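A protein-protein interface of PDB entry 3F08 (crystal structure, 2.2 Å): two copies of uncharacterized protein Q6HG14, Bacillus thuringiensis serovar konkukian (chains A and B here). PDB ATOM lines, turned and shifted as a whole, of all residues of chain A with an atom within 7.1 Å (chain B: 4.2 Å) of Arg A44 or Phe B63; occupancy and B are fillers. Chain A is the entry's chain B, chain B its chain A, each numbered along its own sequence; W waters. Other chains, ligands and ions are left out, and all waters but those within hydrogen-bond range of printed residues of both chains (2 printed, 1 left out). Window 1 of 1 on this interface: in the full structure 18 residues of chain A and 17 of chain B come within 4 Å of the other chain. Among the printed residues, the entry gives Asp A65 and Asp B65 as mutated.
Of the 10 printed residues of chain B, 8 touch a printed residue of chain A. Printed residues of chain B that touch a printed residue of chain A: Trp B18, Gln B19, Gly B22, Gly B23, Val B62, Phe B63, Asn B64 and Asp B65. Hydrophobic or aromatic side chains of chain B within 4 Å of the printed part of chain A: Val B62 and Phe B63. Of the 19 printed residues of chain A, 7 touch a printed residue of chain B. Hydrophobic or aromatic side chains of chain A that line the printed part of chain B: Leu A60, Val A62 and Phe A63. Along chain A the printed residues that touch a printed residue of chain B span positions 41 to 63. Among the printed residues, 16 pairs touch across the chains. Among the printed residues, no Asp or Glu carboxylate lies within 4 Å of a Lys or Arg side-chain nitrogen of the other chain.
The indole nitrogen (NE1) of Trp B18 is in hydrogen-bond range of the side-chain carboxylate (OD1) of Asp B65 (2.9 Å). The backbone carbonyl oxygen (O) of Tyr B69 lies within hydrogen-bond range of the backbone NH (N) of Asn B64, at 3.0 Å. The backbone carbonyl oxygen (O) of Glu A41 is in hydrogen-bond range of the guanidinium group (NE) of Arg A44, 2.9 Å away. The guanidinium group (NH2) of Arg A59 is in salt-bridge range of the side-chain carboxylate (OE1) of Glu A41, 2.6 Å away. The backbone carbonyl oxygen (O) of Arg A44 sits at hydrogen-bond distance from the backbone NH (N) of Leu A60 (2.8 Å). O of Val A62 sits at hydrogen-bond distance from N of Thr A71 (2.8 Å).
Arg A44 touches five residues of chain B. Phe B63 touches just these residues of chain A: Arg A44, Leu A60, Glu A61, Val A62 and Phe A63. Printed residues of chain A within 4 Å of Val B62: Phe A63. Of the printed residues of chain A, Asp B65 touches Leu A60 and Glu A61. Asp A65 touches none of the printed residues of chain B.
CA of Gly B23 touches O of Glu A41 (3.8 Å). Gly B23 touches Gly A42. Arg A44 touches Gly B22 (NH1 to CA, 3.5 Å). CZ of Phe B63 touches CG of Arg A44 (3.7 Å). CE1 of Phe B63 touches O of Leu A60, at 3.4 Å. Asp B65 touches Leu A60 (CB to O, 3.8 Å). Phe B63 touches Glu A61 (CE1 to O, 3.8 Å). Glu A61 touches Asn B64 (O to CA, 3.5 Å). O of Phe B63 touches CA of Val A62, at 3.1 Å. Val B62 touches Phe A63 (CA to O, 3.2 Å).
Val A62 touches Phe B63, and with the chains exchanged Phe A63 touches Val B62. Phe A63 touches its own counterpart, Phe B63. Positions printed for both chains: 62, 63, 64, 65 and 69.
The guanidinium group (NH1) of Arg A44 sits at hydrogen-bond distance from the backbone carbonyl oxygen (O) of Trp B18 (2.8 Å). The side-chain carboxylate (OE1) of Glu A41 sits at hydrogen-bond distance from the side-chain amide nitrogen (NE2) of Gln B19, 2.9 Å away. NH2 of Arg A44 is in hydrogen-bond range of O of Gln B19 (2.8 Å). The backbone carbonyl oxygen (O) of Phe B63 sits at hydrogen-bond distance from the backbone NH (N) of Phe A63 (2.8 Å). The backbone carbonyl oxygen (O) of Glu A61 sits at hydrogen-bond distance from the backbone NH (N) of Asp B65 (2.8 Å). The guanidinium group (NE) of Arg A44 sits close to the backbone NH (N) of Gly B23, 3.3 Å away.
Water W2 bridges OD2 of Asp B65 (2.5 Å) and OE1 of Glu A61 (2.8 Å). Water W1 lies within hydrogen-bond range of the guanidinium group (NE) of Arg A59, the backbone carbonyl oxygen (O) of Leu A60 and the side-chain carboxylate (OD1) of Asp B65.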
ATOM      1  N   PHE A  24      -3.516  27.814  -3.489  1.00  0.00           N
ATOM      2  CA  PHE A  24      -2.325  27.050  -3.807  1.00  0.00           C
ATOM      3  C   PHE A  24      -2.673  25.584  -4.068  1.00  0.00           C
ATOM      4  O   PHE A  24      -2.031  24.924  -4.885  1.00  0.00           O
ATOM      5  CB  PHE A  24      -1.312  27.178  -2.671  1.00  0.00           C
ATOM      6  CG  PHE A  24       0.070  26.715  -3.035  1.00  0.00           C
ATOM      7  CD1 PHE A  24       0.719  27.233  -4.156  1.00  0.00           C
ATOM      8  CD2 PHE A  24       0.729  25.775  -2.252  1.00  0.00           C
ATOM      9  CE1 PHE A  24       2.014  26.818  -4.494  1.00  0.00           C
ATOM     10  CE2 PHE A  24       2.024  25.351  -2.571  1.00  0.00           C
ATOM     11  CZ  PHE A  24       2.664  25.874  -3.696  1.00  0.00           C
ATOM     12  N   LEU A  39      -2.205  19.363   0.379  1.00  0.00           N
ATOM     13  CA  LEU A  39      -1.233  20.249   1.008  1.00  0.00           C
ATOM     14  C   LEU A  39      -0.568  19.626   2.234  1.00  0.00           C
ATOM     15  O   LEU A  39      -1.203  18.872   2.975  1.00  0.00           O
ATOM     16  CB  LEU A  39      -1.911  21.557   1.442  1.00  0.00           C
ATOM     17  CG  LEU A  39      -2.591  22.455   0.403  1.00  0.00           C
ATOM     18  CD1 LEU A  39      -3.431  23.490   1.131  1.00  0.00           C
ATOM     19  CD2 LEU A  39      -1.559  23.136  -0.488  1.00  0.00           C
ATOM     20  N   THR A  40       0.713  19.936   2.434  1.00  0.00           N
ATOM     21  CA  THR A  40       1.437  19.462   3.608  1.00  0.00           C
ATOM     22  C   THR A  40       2.135  20.671   4.215  1.00  0.00           C
ATOM     23  O   THR A  40       2.016  21.784   3.695  1.00  0.00           O
ATOM     24  CB  THR A  40       2.487  18.366   3.275  1.00  0.00           C
ATOM     25  OG1 THR A  40       3.422  18.854   2.310  1.00  0.00           O
ATOM     26  CG2 THR A  40       1.800  17.127   2.738  1.00  0.00           C
ATOM     27  N   GLU A  41       2.840  20.462   5.322  1.00  0.00           N
ATOM     28  CA  GLU A  41       3.532  21.557   5.989  1.00  0.00           C
ATOM     29  C   GLU A  41       2.618  22.752   6.298  1.00  0.00           C
ATOM     30  O   GLU A  41       2.972  23.913   6.059  1.00  0.00           O
ATOM     31  CB  GLU A  41       4.737  21.991   5.146  1.00  0.00           C
ATOM     32  CG  GLU A  41       5.870  20.971   5.185  1.00  0.00           C
ATOM     33  CD  GLU A  41       7.188  21.515   4.674  1.00  0.00           C
ATOM     34  OE1 GLU A  41       7.531  22.673   4.997  1.00  0.00           O
ATOM     35  OE2 GLU A  41       7.890  20.774   3.964  1.00  0.00           O
ATOM     36  N   GLY A  42       1.435  22.452   6.829  1.00  0.00           N
ATOM     37  CA  GLY A  42       0.487  23.489   7.184  1.00  0.00           C
ATOM     38  C   GLY A  42      -0.095  24.267   6.013  1.00  0.00           C
ATOM     39  O   GLY A  42      -0.770  25.278   6.220  1.00  0.00           O
ATOM     40  N   GLY A  43       0.158  23.802   4.791  1.00  0.00           N
ATOM     41  CA  GLY A  43      -0.358  24.480   3.613  1.00  0.00           C
ATOM     42  C   GLY A  43       0.705  25.129   2.742  1.00  0.00           C
ATOM     43  O   GLY A  43       0.384  25.769   1.733  1.00  0.00           O
ATOM     44  N   ARG A  44       1.972  24.958   3.121  1.00  0.00           N
ATOM     45  CA  ARG A  44       3.099  25.535   2.384  1.00  0.00           C
ATOM     46  C   ARG A  44       3.619  24.676   1.232  1.00  0.00           C
ATOM     47  O   ARG A  44       4.371  25.155   0.385  1.00  0.00           O
ATOM     48  CB  ARG A  44       4.263  25.809   3.343  1.00  0.00           C
ATOM     49  CG  ARG A  44       4.065  26.989   4.271  1.00  0.00           C
ATOM     50  CD  ARG A  44       5.169  27.037   5.323  1.00  0.00           C
ATOM     51  NE  ARG A  44       4.977  26.004   6.338  1.00  0.00           N
ATOM     52  CZ  ARG A  44       5.767  25.823   7.393  1.00  0.00           C
ATOM     53  NH1 ARG A  44       6.824  26.598   7.582  1.00  0.00           N
ATOM     54  NH2 ARG A  44       5.482  24.879   8.275  1.00  0.00           N
ATOM     55  N   VAL A  45       3.232  23.409   1.204  1.00  0.00           N
ATOM     56  CA  VAL A  45       3.705  22.513   0.163  1.00  0.00           C
ATOM     57  C   VAL A  45       2.529  21.798  -0.486  1.00  0.00           C
ATOM     58  O   VAL A  45       1.614  21.337   0.206  1.00  0.00           O
ATOM     59  CB  VAL A  45       4.697  21.476   0.764  1.00  0.00           C
ATOM     60  CG1 VAL A  45       5.113  20.459  -0.287  1.00  0.00           C
ATOM     61  CG2 VAL A  45       5.934  22.197   1.307  1.00  0.00           C
ATOM     62  N   ARG A  46       2.531  21.732  -1.812  1.00  0.00           N
ATOM     63  CA  ARG A  46       1.451  21.052  -2.503  1.00  0.00           C
ATOM     64  C   ARG A  46       1.973  19.843  -3.259  1.00  0.00           C
ATOM     65  O   ARG A  46       3.030  19.890  -3.890  1.00  0.00           O
ATOM     66  CB  ARG A  46       0.704  22.007  -3.457  1.00  0.00           C
ATOM     67  CG  ARG A  46       1.502  22.536  -4.635  1.00  0.00           C
ATOM     68  CD  ARG A  46       0.678  23.557  -5.413  1.00  0.00           C
ATOM     69  NE  ARG A  46       1.411  24.134  -6.542  1.00  0.00           N
ATOM     70  CZ  ARG A  46       0.984  25.170  -7.260  1.00  0.00           C
ATOM     71  NH1 ARG A  46      -0.179  25.750  -6.973  1.00  0.00           N
ATOM     72  NH2 ARG A  46       1.719  25.633  -8.266  1.00  0.00           N
ATOM     73  N   GLU A  58       5.637  20.977  -4.914  1.00  0.00           N
ATOM     74  CA  GLU A  58       6.016  22.372  -5.078  1.00  0.00           C
ATOM     75  C   GLU A  58       5.882  23.125  -3.764  1.00  0.00           C
ATOM     76  O   GLU A  58       5.002  22.841  -2.953  1.00  0.00           O
ATOM     77  CB  GLU A  58       5.153  23.016  -6.164  1.00  0.00           C
ATOM     78  CG  GLU A  58       5.099  22.179  -7.434  1.00  0.00           C
ATOM     79  CD  GLU A  58       4.354  22.848  -8.569  1.00  0.00           C
ATOM     80  OE1 GLU A  58       3.401  23.613  -8.301  1.00  0.00           O
ATOM     81  OE2 GLU A  58       4.710  22.586  -9.741  1.00  0.00           O
ATOM     82  N   ARG A  59       6.758  24.099  -3.570  1.00  0.00           N
ATOM     83  CA  ARG A  59       6.776  24.873  -2.345  1.00  0.00           C
ATOM     84  C   ARG A  59       6.283  26.307  -2.524  1.00  0.00           C
ATOM     85  O   ARG A  59       6.681  26.993  -3.470  1.00  0.00           O
ATOM     86  CB  ARG A  59       8.204  24.856  -1.794  1.00  0.00           C
ATOM     87  CG  ARG A  59       8.499  25.904  -0.763  1.00  0.00           C
ATOM     88  CD  ARG A  59       9.579  25.443   0.195  1.00  0.00           C
ATOM     89  NE  ARG A  59       9.023  25.522   1.531  1.00  0.00           N
ATOM     90  CZ  ARG A  59       8.922  24.505   2.374  1.00  0.00           C
ATOM     91  NH1 ARG A  59       9.358  23.299   2.039  1.00  0.00           N
ATOM     92  NH2 ARG A  59       8.353  24.703   3.549  1.00  0.00           N
ATOM     93  N   LEU A  60       5.394  26.739  -1.631  1.00  0.00           N
ATOM     94  CA  LEU A  60       4.873  28.104  -1.671  1.00  0.00           C
ATOM     95  C   LEU A  60       5.975  29.048  -1.183  1.00  0.00           C
ATOM     96  O   LEU A  60       6.489  28.874  -0.072  1.00  0.00           O
ATOM     97  CB  LEU A  60       3.647  28.244  -0.759  1.00  0.00           C
ATOM     98  CG  LEU A  60       3.012  29.643  -0.685  1.00  0.00           C
ATOM     99  CD1 LEU A  60       2.377  29.985  -2.038  1.00  0.00           C
ATOM    100  CD2 LEU A  60       1.959  29.692   0.419  1.00  0.00           C
ATOM    101  N   GLU A  61       6.339  30.038  -1.997  1.00  0.00           N
ATOM    102  CA  GLU A  61       7.391  30.980  -1.614  1.00  0.00           C
ATOM    103  C   GLU A  61       6.835  32.333  -1.185  1.00  0.00           C
ATOM    104  O   GLU A  61       7.272  32.905  -0.183  1.00  0.00           O
ATOM    105  CB  GLU A  61       8.371  31.194  -2.769  1.00  0.00           C
ATOM    106  CG  GLU A  61       9.184  29.970  -3.179  1.00  0.00           C
ATOM    107  CD  GLU A  61      10.182  29.533  -2.117  1.00  0.00           C
ATOM    108  OE1 GLU A  61      10.509  30.351  -1.228  1.00  0.00           O
ATOM    109  OE2 GLU A  61      10.649  28.375  -2.182  1.00  0.00           O
ATOM    110  N   VAL A  62       5.891  32.851  -1.965  1.00  0.00           N
ATOM    111  CA  VAL A  62       5.265  34.130  -1.677  1.00  0.00           C
ATOM    112  C   VAL A  62       3.789  34.057  -2.025  1.00  0.00           C
ATOM    113  O   VAL A  62       3.387  33.361  -2.961  1.00  0.00           O
ATOM    114  CB  VAL A  62       5.882  35.292  -2.516  1.00  0.00           C
ATOM    115  CG1 VAL A  62       5.359  36.625  -2.008  1.00  0.00           C
ATOM    116  CG2 VAL A  62       7.415  35.270  -2.441  1.00  0.00           C
ATOM    117  N   PHE A  63       2.983  34.778  -1.264  1.00  0.00           N
ATOM    118  CA  PHE A  63       1.558  34.845  -1.513  1.00  0.00           C
ATOM    119  C   PHE A  63       1.085  36.232  -1.118  1.00  0.00           C
ATOM    120  O   PHE A  63       1.476  36.754  -0.072  1.00  0.00           O
ATOM    121  CB  PHE A  63       0.808  33.783  -0.701  1.00  0.00           C
ATOM    122  CG  PHE A  63      -0.689  33.880  -0.810  1.00  0.00           C
ATOM    123  CD1 PHE A  63      -1.411  34.749   0.009  1.00  0.00           C
ATOM    124  CD2 PHE A  63      -1.379  33.119  -1.753  1.00  0.00           C
ATOM    125  CE1 PHE A  63      -2.813  34.860  -0.109  1.00  0.00           C
ATOM    126  CE2 PHE A  63      -2.771  33.217  -1.882  1.00  0.00           C
ATOM    127  CZ  PHE A  63      -3.490  34.089  -1.059  1.00  0.00           C
ATOM    128  N   ASN A  64       0.261  36.837  -1.966  1.00  0.00           N
ATOM    129  CA  ASN A  64      -0.275  38.160  -1.685  1.00  0.00           C
ATOM    130  C   ASN A  64      -1.682  38.181  -2.249  1.00  0.00           C
ATOM    131  O   ASN A  64      -1.867  38.234  -3.467  1.00  0.00           O
ATOM    132  CB  ASN A  64       0.584  39.249  -2.332  1.00  0.00           C
ATOM    133  CG  ASN A  64       0.286  40.627  -1.771  1.00  0.00           C
ATOM    134  OD1 ASN A  64       1.198  41.385  -1.438  1.00  0.00           O
ATOM    135  ND2 ASN A  64      -0.992  40.960  -1.663  1.00  0.00           N
ATOM    136  N   ASP A  65      -2.670  38.125  -1.357  1.00  0.00           N
ATOM    137  CA  ASP A  65      -4.072  38.092  -1.769  1.00  0.00           C
ATOM    138  C   ASP A  65      -4.545  39.323  -2.536  1.00  0.00           C
ATOM    139  O   ASP A  65      -5.165  39.202  -3.592  1.00  0.00           O
ATOM    140  CB  ASP A  65      -4.984  37.872  -0.552  1.00  0.00           C
ATOM    141  CG  ASP A  65      -6.411  37.510  -0.946  1.00  0.00           C
ATOM    142  OD1 ASP A  65      -6.606  36.460  -1.600  1.00  0.00           O
ATOM    143  OD2 ASP A  65      -7.339  38.272  -0.602  1.00  0.00           O
ATOM    144  N   TYR A  69      -1.300  37.279  -6.499  1.00  0.00           N
ATOM    145  CA  TYR A  69      -0.253  36.460  -7.083  1.00  0.00           C
ATOM    146  C   TYR A  69       0.362  35.560  -6.022  1.00  0.00           C
ATOM    147  O   TYR A  69       0.228  35.817  -4.822  1.00  0.00           O
ATOM    148  CB  TYR A  69       0.836  37.342  -7.715  1.00  0.00           C
ATOM    149  CG  TYR A  69       1.806  37.968  -6.733  1.00  0.00           C
ATOM    150  CD1 TYR A  69       2.933  37.274  -6.302  1.00  0.00           C
ATOM    151  CD2 TYR A  69       1.611  39.263  -6.259  1.00  0.00           C
ATOM    152  CE1 TYR A  69       3.850  37.855  -5.425  1.00  0.00           C
ATOM    153  CE2 TYR A  69       2.520  39.859  -5.383  1.00  0.00           C
ATOM    154  CZ  TYR A  69       3.638  39.149  -4.971  1.00  0.00           C
ATOM    155  OH  TYR A  69       4.551  39.736  -4.123  1.00  0.00           O
ATOM    156  N   THR A  71       3.976  32.815  -5.619  1.00  0.00           N
ATOM    157  CA  THR A  71       5.222  32.372  -6.210  1.00  0.00           C
ATOM    158  C   THR A  71       5.575  31.040  -5.591  1.00  0.00           C
ATOM    159  O   THR A  71       5.451  30.861  -4.382  1.00  0.00           O
ATOM    160  CB  THR A  71       6.345  33.389  -5.913  1.00  0.00           C
ATOM    161  OG1 THR A  71       5.968  34.670  -6.435  1.00  0.00           O
ATOM    162  CG2 THR A  71       7.675  32.942  -6.536  1.00  0.00           C
ATOM    163  N   TRP B  18      10.514  28.683  12.139  1.00  0.00           N
ATOM    164  CA  TRP B  18       9.657  28.913  10.983  1.00  0.00           C
ATOM    165  C   TRP B  18       9.065  27.602  10.478  1.00  0.00           C
ATOM    166  O   TRP B  18       7.930  27.569  10.012  1.00  0.00           O
ATOM    167  CB  TRP B  18      10.440  29.581   9.857  1.00  0.00           C
ATOM    168  CG  TRP B  18       9.584  29.955   8.676  1.00  0.00           C
ATOM    169  CD1 TRP B  18       9.753  29.553   7.379  1.00  0.00           C
ATOM    170  CD2 TRP B  18       8.444  30.832   8.681  1.00  0.00           C
ATOM    171  NE1 TRP B  18       8.789  30.130   6.578  1.00  0.00           N
ATOM    172  CE2 TRP B  18       7.976  30.917   7.350  1.00  0.00           C
ATOM    173  CE3 TRP B  18       7.775  31.551   9.680  1.00  0.00           C
ATOM    174  CZ2 TRP B  18       6.864  31.696   6.994  1.00  0.00           C
ATOM    175  CZ3 TRP B  18       6.669  32.327   9.324  1.00  0.00           C
ATOM    176  CH2 TRP B  18       6.227  32.392   7.991  1.00  0.00           C
ATOM    177  N   GLN B  19       9.831  26.521  10.569  1.00  0.00           N
ATOM    178  CA  GLN B  19       9.330  25.233  10.113  1.00  0.00           C
ATOM    179  C   GLN B  19       8.095  24.843  10.921  1.00  0.00           C
ATOM    180  O   GLN B  19       7.165  24.228  10.403  1.00  0.00           O
ATOM    181  CB  GLN B  19      10.397  24.145  10.254  1.00  0.00           C
ATOM    182  CG  GLN B  19       9.981  22.828   9.612  1.00  0.00           C
ATOM    183  CD  GLN B  19       9.665  22.985   8.125  1.00  0.00           C
ATOM    184  OE1 GLN B  19      10.562  23.182   7.300  1.00  0.00           O
ATOM    185  NE2 GLN B  19       8.385  22.909   7.780  1.00  0.00           N
ATOM    186  N   GLY B  22       5.331  28.483  10.561  1.00  0.00           N
ATOM    187  CA  GLY B  22       5.064  29.109   9.273  1.00  0.00           C
ATOM    188  C   GLY B  22       3.816  28.672   8.522  1.00  0.00           C
ATOM    189  O   GLY B  22       3.288  29.424   7.710  1.00  0.00           O
ATOM    190  N   GLY B  23       3.340  27.459   8.782  1.00  0.00           N
ATOM    191  CA  GLY B  23       2.157  26.963   8.097  1.00  0.00           C
ATOM    192  C   GLY B  23       0.871  27.596   8.596  1.00  0.00           C
ATOM    193  O   GLY B  23       0.634  27.699   9.801  1.00  0.00           O
ATOM    194  N   VAL B  62      -0.953  37.716   3.310  1.00  0.00           N
ATOM    195  CA  VAL B  62       0.389  37.749   2.750  1.00  0.00           C
ATOM    196  C   VAL B  62       1.220  36.628   3.345  1.00  0.00           C
ATOM    197  O   VAL B  62       1.031  36.250   4.504  1.00  0.00           O
ATOM    198  CB  VAL B  62       1.115  39.089   3.073  1.00  0.00           C
ATOM    199  CG1 VAL B  62       2.446  39.139   2.350  1.00  0.00           C
ATOM    200  CG2 VAL B  62       0.256  40.267   2.677  1.00  0.00           C
ATOM    201  N   PHE B  63       2.133  36.096   2.539  1.00  0.00           N
ATOM    202  CA  PHE B  63       3.033  35.040   2.985  1.00  0.00           C
ATOM    203  C   PHE B  63       4.358  35.153   2.254  1.00  0.00           C
ATOM    204  O   PHE B  63       4.397  35.305   1.039  1.00  0.00           O
ATOM    205  CB  PHE B  63       2.429  33.653   2.734  1.00  0.00           C
ATOM    206  CG  PHE B  63       3.385  32.514   3.007  1.00  0.00           C
ATOM    207  CD1 PHE B  63       4.219  32.019   2.001  1.00  0.00           C
ATOM    208  CD2 PHE B  63       3.467  31.954   4.282  1.00  0.00           C
ATOM    209  CE1 PHE B  63       5.129  30.975   2.266  1.00  0.00           C
ATOM    210  CE2 PHE B  63       4.366  30.914   4.561  1.00  0.00           C
ATOM    211  CZ  PHE B  63       5.201  30.421   3.554  1.00  0.00           C
ATOM    212  N   ASN B  64       5.449  35.081   3.002  1.00  0.00           N
ATOM    213  CA  ASN B  64       6.770  35.158   2.396  1.00  0.00           C
ATOM    214  C   ASN B  64       7.675  34.194   3.153  1.00  0.00           C
ATOM    215  O   ASN B  64       8.076  34.465   4.285  1.00  0.00           O
ATOM    216  CB  ASN B  64       7.297  36.592   2.489  1.00  0.00           C
ATOM    217  CG  ASN B  64       8.542  36.806   1.661  1.00  0.00           C
ATOM    218  OD1 ASN B  64       9.537  36.095   1.817  1.00  0.00           O
ATOM    219  ND2 ASN B  64       8.494  37.790   0.770  1.00  0.00           N
ATOM    220  N   ASP B  65       7.989  33.068   2.521  1.00  0.00           N
ATOM    221  CA  ASP B  65       8.821  32.044   3.137  1.00  0.00           C
ATOM    222  C   ASP B  65      10.244  32.509   3.459  1.00  0.00           C
ATOM    223  O   ASP B  65      10.766  32.238   4.547  1.00  0.00           O
ATOM    224  CB  ASP B  65       8.881  30.815   2.228  1.00  0.00           C
ATOM    225  CG  ASP B  65       9.453  29.604   2.927  1.00  0.00           C
ATOM    226  OD1 ASP B  65       8.816  29.100   3.880  1.00  0.00           O
ATOM    227  OD2 ASP B  65      10.548  29.153   2.530  1.00  0.00           O
ATOM    228  N   TYR B  69       7.400  35.294   7.304  1.00  0.00           N
ATOM    229  CA  TYR B  69       6.277  35.946   7.947  1.00  0.00           C
ATOM    230  C   TYR B  69       5.017  35.707   7.146  1.00  0.00           C
ATOM    231  O   TYR B  69       5.083  35.398   5.958  1.00  0.00           O
ATOM    232  CB  TYR B  69       6.524  37.454   8.080  1.00  0.00           C
ATOM    233  CG  TYR B  69       6.299  38.250   6.810  1.00  0.00           C
ATOM    234  CD1 TYR B  69       5.029  38.727   6.478  1.00  0.00           C
ATOM    235  CD2 TYR B  69       7.356  38.557   5.959  1.00  0.00           C
ATOM    236  CE1 TYR B  69       4.822  39.501   5.336  1.00  0.00           C
ATOM    237  CE2 TYR B  69       7.159  39.325   4.816  1.00  0.00           C
ATOM    238  CZ  TYR B  69       5.895  39.796   4.512  1.00  0.00           C
ATOM    239  OH  TYR B  69       5.717  40.580   3.402  1.00  0.00           O
ATOM    240  N   TYR B  70       3.872  35.793   7.816  1.00  0.00           N
ATOM    241  CA  TYR B  70       2.600  35.686   7.129  1.00  0.00           C
ATOM    242  C   TYR B  70       1.659  36.650   7.831  1.00  0.00           C
ATOM    243  O   TYR B  70       1.787  36.903   9.030  1.00  0.00           O
ATOM    244  CB  TYR B  70       2.072  34.231   7.079  1.00  0.00           C
ATOM    245  CG  TYR B  70       1.547  33.593   8.349  1.00  0.00           C
ATOM    246  CD1 TYR B  70       0.270  33.889   8.835  1.00  0.00           C
ATOM    247  CD2 TYR B  70       2.279  32.601   8.997  1.00  0.00           C
ATOM    248  CE1 TYR B  70      -0.268  33.193   9.938  1.00  0.00           C
ATOM    249  CE2 TYR B  70       1.757  31.904  10.093  1.00  0.00           C
ATOM    250  CZ  TYR B  70       0.487  32.202  10.556  1.00  0.00           C
ATOM    251  OH  TYR B  70      -0.014  31.494  11.624  1.00  0.00           O
HETATM  252  O   HOH W   1       7.109  27.381   2.294  1.00  0.00           O
HETATM  253  O   HOH W   2      12.127  28.929   0.554  1.00  0.00           O
